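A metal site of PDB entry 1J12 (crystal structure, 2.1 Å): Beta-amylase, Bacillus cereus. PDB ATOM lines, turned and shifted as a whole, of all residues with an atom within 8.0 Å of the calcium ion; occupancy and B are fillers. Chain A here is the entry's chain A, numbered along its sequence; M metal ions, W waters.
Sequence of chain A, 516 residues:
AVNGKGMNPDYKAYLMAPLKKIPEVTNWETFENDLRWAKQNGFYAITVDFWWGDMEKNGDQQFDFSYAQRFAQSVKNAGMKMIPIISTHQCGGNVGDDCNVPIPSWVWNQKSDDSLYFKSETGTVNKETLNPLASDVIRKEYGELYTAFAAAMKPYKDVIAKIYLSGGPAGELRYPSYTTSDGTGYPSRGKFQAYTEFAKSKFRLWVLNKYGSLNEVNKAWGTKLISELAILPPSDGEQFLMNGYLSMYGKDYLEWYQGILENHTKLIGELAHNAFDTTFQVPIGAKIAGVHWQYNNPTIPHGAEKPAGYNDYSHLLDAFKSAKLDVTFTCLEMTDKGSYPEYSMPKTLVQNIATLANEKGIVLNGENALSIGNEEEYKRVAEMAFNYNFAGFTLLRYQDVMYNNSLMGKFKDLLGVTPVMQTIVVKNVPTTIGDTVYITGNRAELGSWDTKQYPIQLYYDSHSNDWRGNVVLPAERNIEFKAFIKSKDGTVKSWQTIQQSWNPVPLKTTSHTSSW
Water W1 lies within hydrogen-bond range of the backbone carbonyl oxygen of Glu 141 (2.6 Å), the side-chain carboxylate of Glu 56 (2.6 Å) and the backbone NH of Leu 145 (3.3 Å).
The side-chain amino group (NZ) of Lys 140 lies within salt-bridge range of the side-chain carboxylate (OE2) of Glu 144, 3.3 Å away. The backbone carbonyl oxygen (O) of Glu 56 is in hydrogen-bond range of the indole nitrogen (NE1) of Trp 106, at 2.9 Å. The side-chain carboxylate (OE1) of Glu 56 is in hydrogen-bond range of the indole nitrogen (NE1) of Trp 52, at 2.9 Å. NZ of Lys 140 lies within salt-bridge range of OD2 of Asp 60, at 3.1 Å. The side-chain amino group of Lys 140 is in salt-bridge range of the side-chain carboxylate of Glu 141 (3.0 Å).
The calcium ion is bound by the side-chain carboxylate (OE1) of Glu 144 (2.3 Å), the side-chain carboxylate (OE2) of Glu 56 (2.4 Å), the side-chain carboxylate (OD1) of Asp 60 (2.4 Å), the side-chain carboxylate (OE1) of Glu 141 (2.6 Å), water W1 (2.6 Å) and the side-chain amide oxygen (OE1) of Gln 61 (2.6 Å).
Within 4 Å of the calcium ion: Glu 56, Asp 60, Gln 61, Glu 141 and Glu 144.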
ATOM      1  N   TRP A  52       9.620 -11.314 -33.701  1.00  0.00           N
ATOM      2  CA  TRP A  52       8.425 -11.601 -32.924  1.00  0.00           C
ATOM      3  C   TRP A  52       8.309 -10.576 -31.794  1.00  0.00           C
ATOM      4  O   TRP A  52       7.221 -10.079 -31.512  1.00  0.00           O
ATOM      5  CB  TRP A  52       8.483 -13.034 -32.372  1.00  0.00           C
ATOM      6  CG  TRP A  52       7.206 -13.500 -31.734  1.00  0.00           C
ATOM      7  CD1 TRP A  52       5.979 -12.914 -31.830  1.00  0.00           C
ATOM      8  CD2 TRP A  52       7.037 -14.648 -30.879  1.00  0.00           C
ATOM      9  NE1 TRP A  52       5.059 -13.607 -31.089  1.00  0.00           N
ATOM     10  CE2 TRP A  52       5.687 -14.677 -30.488  1.00  0.00           C
ATOM     11  CE3 TRP A  52       7.902 -15.645 -30.396  1.00  0.00           C
ATOM     12  CZ2 TRP A  52       5.169 -15.659 -29.648  1.00  0.00           C
ATOM     13  CZ3 TRP A  52       7.390 -16.623 -29.564  1.00  0.00           C
ATOM     14  CH2 TRP A  52       6.036 -16.634 -29.195  1.00  0.00           C
ATOM     15  N   GLU A  56       4.484  -8.515 -31.746  1.00  0.00           N
ATOM     16  CA  GLU A  56       3.468  -8.877 -30.754  1.00  0.00           C
ATOM     17  C   GLU A  56       4.040  -8.584 -29.369  1.00  0.00           C
ATOM     18  O   GLU A  56       3.847  -9.347 -28.424  1.00  0.00           O
ATOM     19  CB  GLU A  56       3.116 -10.366 -30.893  1.00  0.00           C
ATOM     20  CG  GLU A  56       1.925 -10.835 -30.069  1.00  0.00           C
ATOM     21  CD  GLU A  56       1.527 -12.275 -30.357  1.00  0.00           C
ATOM     22  OE1 GLU A  56       2.195 -12.974 -31.146  1.00  0.00           O
ATOM     23  OE2 GLU A  56       0.514 -12.724 -29.787  1.00  0.00           O
ATOM     24  N   GLY A  59       1.484  -7.488 -25.864  1.00  0.00           N
ATOM     25  CA  GLY A  59       0.629  -8.524 -25.323  1.00  0.00           C
ATOM     26  C   GLY A  59       0.054  -9.474 -26.333  1.00  0.00           C
ATOM     27  O   GLY A  59       0.183  -9.263 -27.533  1.00  0.00           O
ATOM     28  N   ASP A  60      -0.587 -10.541 -25.838  1.00  0.00           N
ATOM     29  CA  ASP A  60      -1.184 -11.553 -26.690  1.00  0.00           C
ATOM     30  C   ASP A  60      -2.186 -10.920 -27.660  1.00  0.00           C
ATOM     31  O   ASP A  60      -3.158 -10.287 -27.243  1.00  0.00           O
ATOM     32  CB  ASP A  60      -1.890 -12.643 -25.855  1.00  0.00           C
ATOM     33  CG  ASP A  60      -2.420 -13.786 -26.709  1.00  0.00           C
ATOM     34  OD1 ASP A  60      -1.882 -14.014 -27.802  1.00  0.00           O
ATOM     35  OD2 ASP A  60      -3.365 -14.485 -26.284  1.00  0.00           O
ATOM     36  N   GLN A  61      -1.943 -11.148 -28.942  1.00  0.00           N
ATOM     37  CA  GLN A  61      -2.771 -10.645 -30.032  1.00  0.00           C
ATOM     38  C   GLN A  61      -2.725  -9.122 -30.183  1.00  0.00           C
ATOM     39  O   GLN A  61      -3.578  -8.528 -30.826  1.00  0.00           O
ATOM     40  CB  GLN A  61      -4.220 -11.148 -29.918  1.00  0.00           C
ATOM     41  CG  GLN A  61      -4.366 -12.672 -29.924  1.00  0.00           C
ATOM     42  CD  GLN A  61      -3.799 -13.329 -31.175  1.00  0.00           C
ATOM     43  OE1 GLN A  61      -2.600 -13.590 -31.271  1.00  0.00           O
ATOM     44  NE2 GLN A  61      -4.656 -13.606 -32.147  1.00  0.00           N
ATOM     45  N   GLN A  62      -1.734  -8.497 -29.548  1.00  0.00           N
ATOM     46  CA  GLN A  62      -1.558  -7.050 -29.671  1.00  0.00           C
ATOM     47  C   GLN A  62      -0.476  -6.857 -30.736  1.00  0.00           C
ATOM     48  O   GLN A  62       0.663  -6.526 -30.429  1.00  0.00           O
ATOM     49  CB  GLN A  62      -1.149  -6.439 -28.332  1.00  0.00           C
ATOM     50  CG  GLN A  62      -2.269  -6.460 -27.317  1.00  0.00           C
ATOM     51  CD  GLN A  62      -1.885  -5.837 -25.994  1.00  0.00           C
ATOM     52  OE1 GLN A  62      -1.280  -4.770 -25.942  1.00  0.00           O
ATOM     53  NE2 GLN A  62      -2.249  -6.509 -24.917  1.00  0.00           N
ATOM     54  N   PHE A  63      -0.872  -7.088 -31.985  1.00  0.00           N
ATOM     55  CA  PHE A  63       0.017  -7.001 -33.138  1.00  0.00           C
ATOM     56  C   PHE A  63       0.389  -5.618 -33.629  1.00  0.00           C
ATOM     57  O   PHE A  63      -0.353  -4.651 -33.440  1.00  0.00           O
ATOM     58  CB  PHE A  63      -0.577  -7.794 -34.310  1.00  0.00           C
ATOM     59  CG  PHE A  63      -0.735  -9.271 -34.026  1.00  0.00           C
ATOM     60  CD1 PHE A  63      -2.000  -9.847 -33.972  1.00  0.00           C
ATOM     61  CD2 PHE A  63       0.384 -10.069 -33.809  1.00  0.00           C
ATOM     62  CE1 PHE A  63      -2.145 -11.210 -33.683  1.00  0.00           C
ATOM     63  CE2 PHE A  63       0.249 -11.421 -33.521  1.00  0.00           C
ATOM     64  CZ  PHE A  63      -1.017 -11.998 -33.468  1.00  0.00           C
ATOM     65  N   TRP A 106       5.678 -11.471 -22.183  1.00  0.00           N
ATOM     66  CA  TRP A 106       4.428 -12.015 -21.637  1.00  0.00           C
ATOM     67  C   TRP A 106       4.326 -13.517 -21.934  1.00  0.00           C
ATOM     68  O   TRP A 106       3.648 -14.236 -21.229  1.00  0.00           O
ATOM     69  CB  TRP A 106       3.197 -11.272 -22.191  1.00  0.00           C
ATOM     70  CG  TRP A 106       3.111 -11.247 -23.691  1.00  0.00           C
ATOM     71  CD1 TRP A 106       3.577 -10.274 -24.522  1.00  0.00           C
ATOM     72  CD2 TRP A 106       2.578 -12.280 -24.541  1.00  0.00           C
ATOM     73  NE1 TRP A 106       3.389 -10.630 -25.834  1.00  0.00           N
ATOM     74  CE2 TRP A 106       2.777 -11.864 -25.882  1.00  0.00           C
ATOM     75  CE3 TRP A 106       1.967 -13.521 -24.311  1.00  0.00           C
ATOM     76  CZ2 TRP A 106       2.392 -12.643 -26.964  1.00  0.00           C
ATOM     77  CZ3 TRP A 106       1.583 -14.300 -25.393  1.00  0.00           C
ATOM     78  CH2 TRP A 106       1.796 -13.856 -26.710  1.00  0.00           C
ATOM     79  N   VAL A 107       5.021 -13.969 -22.972  1.00  0.00           N
ATOM     80  CA  VAL A 107       5.011 -15.375 -23.358  1.00  0.00           C
ATOM     81  C   VAL A 107       5.471 -16.288 -22.233  1.00  0.00           C
ATOM     82  O   VAL A 107       4.881 -17.344 -22.003  1.00  0.00           O
ATOM     83  CB  VAL A 107       5.872 -15.626 -24.609  1.00  0.00           C
ATOM     84  CG1 VAL A 107       5.900 -17.102 -24.968  1.00  0.00           C
ATOM     85  CG2 VAL A 107       5.311 -14.850 -25.776  1.00  0.00           C
ATOM     86  N   GLN A 110       3.007 -17.580 -19.595  1.00  0.00           N
ATOM     87  CA  GLN A 110       1.982 -18.528 -20.019  1.00  0.00           C
ATOM     88  C   GLN A 110       2.075 -19.884 -19.327  1.00  0.00           C
ATOM     89  O   GLN A 110       1.106 -20.655 -19.325  1.00  0.00           O
ATOM     90  CB  GLN A 110       2.048 -18.726 -21.547  1.00  0.00           C
ATOM     91  CG  GLN A 110       1.957 -17.451 -22.378  1.00  0.00           C
ATOM     92  CD  GLN A 110       0.587 -16.809 -22.348  1.00  0.00           C
ATOM     93  OE1 GLN A 110       0.361 -15.816 -21.652  1.00  0.00           O
ATOM     94  NE2 GLN A 110      -0.334 -17.355 -23.123  1.00  0.00           N
ATOM     95  N   VAL A 137       1.840 -24.522 -26.688  1.00  0.00           N
ATOM     96  CA  VAL A 137       2.059 -23.086 -26.674  1.00  0.00           C
ATOM     97  C   VAL A 137       2.472 -22.665 -28.086  1.00  0.00           C
ATOM     98  O   VAL A 137       1.970 -21.685 -28.640  1.00  0.00           O
ATOM     99  CB  VAL A 137       3.171 -22.719 -25.665  1.00  0.00           C
ATOM    100  CG1 VAL A 137       3.485 -21.232 -25.704  1.00  0.00           C
ATOM    101  CG2 VAL A 137       2.779 -23.169 -24.263  1.00  0.00           C
ATOM    102  N   LYS A 140      -0.411 -22.693 -30.614  1.00  0.00           N
ATOM    103  CA  LYS A 140      -1.238 -21.502 -30.424  1.00  0.00           C
ATOM    104  C   LYS A 140      -0.571 -20.227 -30.917  1.00  0.00           C
ATOM    105  O   LYS A 140      -1.093 -19.540 -31.797  1.00  0.00           O
ATOM    106  CB  LYS A 140      -1.591 -21.309 -28.948  1.00  0.00           C
ATOM    107  CG  LYS A 140      -2.332 -19.989 -28.663  1.00  0.00           C
ATOM    108  CD  LYS A 140      -2.656 -19.794 -27.190  1.00  0.00           C
ATOM    109  CE  LYS A 140      -3.394 -18.473 -26.943  1.00  0.00           C
ATOM    110  NZ  LYS A 140      -2.586 -17.267 -27.288  1.00  0.00           N
ATOM    111  N   GLU A 141       0.585 -19.911 -30.350  1.00  0.00           N
ATOM    112  CA  GLU A 141       1.293 -18.688 -30.686  1.00  0.00           C
ATOM    113  C   GLU A 141       1.797 -18.539 -32.114  1.00  0.00           C
ATOM    114  O   GLU A 141       1.632 -17.481 -32.720  1.00  0.00           O
ATOM    115  CB  GLU A 141       2.427 -18.458 -29.678  1.00  0.00           C
ATOM    116  CG  GLU A 141       1.963 -18.493 -28.211  1.00  0.00           C
ATOM    117  CD  GLU A 141       0.933 -17.408 -27.850  1.00  0.00           C
ATOM    118  OE1 GLU A 141       0.724 -16.452 -28.626  1.00  0.00           O
ATOM    119  OE2 GLU A 141       0.347 -17.502 -26.742  1.00  0.00           O
ATOM    120  N   TYR A 142       2.391 -19.600 -32.672  1.00  0.00           N
ATOM    121  CA  TYR A 142       2.881 -19.535 -34.040  1.00  0.00           C
ATOM    122  C   TYR A 142       1.710 -19.530 -35.005  1.00  0.00           C
ATOM    123  O   TYR A 142       1.716 -18.815 -35.996  1.00  0.00           O
ATOM    124  CB  TYR A 142       3.804 -20.729 -34.370  1.00  0.00           C
ATOM    125  CG  TYR A 142       5.190 -20.659 -33.767  1.00  0.00           C
ATOM    126  CD1 TYR A 142       5.427 -20.005 -32.559  1.00  0.00           C
ATOM    127  CD2 TYR A 142       6.260 -21.270 -34.406  1.00  0.00           C
ATOM    128  CE1 TYR A 142       6.705 -19.959 -32.010  1.00  0.00           C
ATOM    129  CE2 TYR A 142       7.541 -21.237 -33.860  1.00  0.00           C
ATOM    130  CZ  TYR A 142       7.759 -20.579 -32.664  1.00  0.00           C
ATOM    131  OH  TYR A 142       9.024 -20.544 -32.144  1.00  0.00           O
ATOM    132  N   GLY A 143       0.709 -20.363 -34.720  1.00  0.00           N
ATOM    133  CA  GLY A 143      -0.459 -20.412 -35.572  1.00  0.00           C
ATOM    134  C   GLY A 143      -1.075 -19.032 -35.659  1.00  0.00           C
ATOM    135  O   GLY A 143      -1.374 -18.546 -36.757  1.00  0.00           O
ATOM    136  N   GLU A 144      -1.193 -18.370 -34.510  1.00  0.00           N
ATOM    137  CA  GLU A 144      -1.760 -17.037 -34.418  1.00  0.00           C
ATOM    138  C   GLU A 144      -0.921 -15.981 -35.110  1.00  0.00           C
ATOM    139  O   GLU A 144      -1.438 -15.127 -35.822  1.00  0.00           O
ATOM    140  CB  GLU A 144      -1.958 -16.641 -32.963  1.00  0.00           C
ATOM    141  CG  GLU A 144      -3.149 -17.305 -32.274  1.00  0.00           C
ATOM    142  CD  GLU A 144      -3.188 -17.040 -30.776  1.00  0.00           C
ATOM    143  OE1 GLU A 144      -2.170 -16.575 -30.201  1.00  0.00           O
ATOM    144  OE2 GLU A 144      -4.225 -17.314 -30.150  1.00  0.00           O
ATOM    145  N   LEU A 145       0.398 -16.047 -34.924  1.00  0.00           N
ATOM    146  CA  LEU A 145       1.308 -15.093 -35.536  1.00  0.00           C
ATOM    147  C   LEU A 145       1.426 -15.258 -37.051  1.00  0.00           C
ATOM    148  O   LEU A 145       1.537 -14.269 -37.763  1.00  0.00           O
ATOM    149  CB  LEU A 145       2.697 -15.194 -34.895  1.00  0.00           C
ATOM    150  CG  LEU A 145       3.787 -14.315 -35.493  1.00  0.00           C
ATOM    151  CD1 LEU A 145       3.541 -12.866 -35.169  1.00  0.00           C
ATOM    152  CD2 LEU A 145       5.139 -14.738 -34.964  1.00  0.00           C
ATOM    153  N   ALA A 148      -1.935 -14.011 -38.627  1.00  0.00           N
ATOM    154  CA  ALA A 148      -2.004 -12.559 -38.551  1.00  0.00           C
ATOM    155  C   ALA A 148      -1.059 -11.900 -39.554  1.00  0.00           C
ATOM    156  O   ALA A 148      -1.420 -10.909 -40.193  1.00  0.00           O
ATOM    157  CB  ALA A 148      -1.697 -12.095 -37.140  1.00  0.00           C
HETATM  158 CA    CA M   1      -0.760 -14.749 -29.815  1.00  0.00          CA
HETATM  159  O   HOH W   1       0.838 -15.151 -31.784  1.00  0.00           O
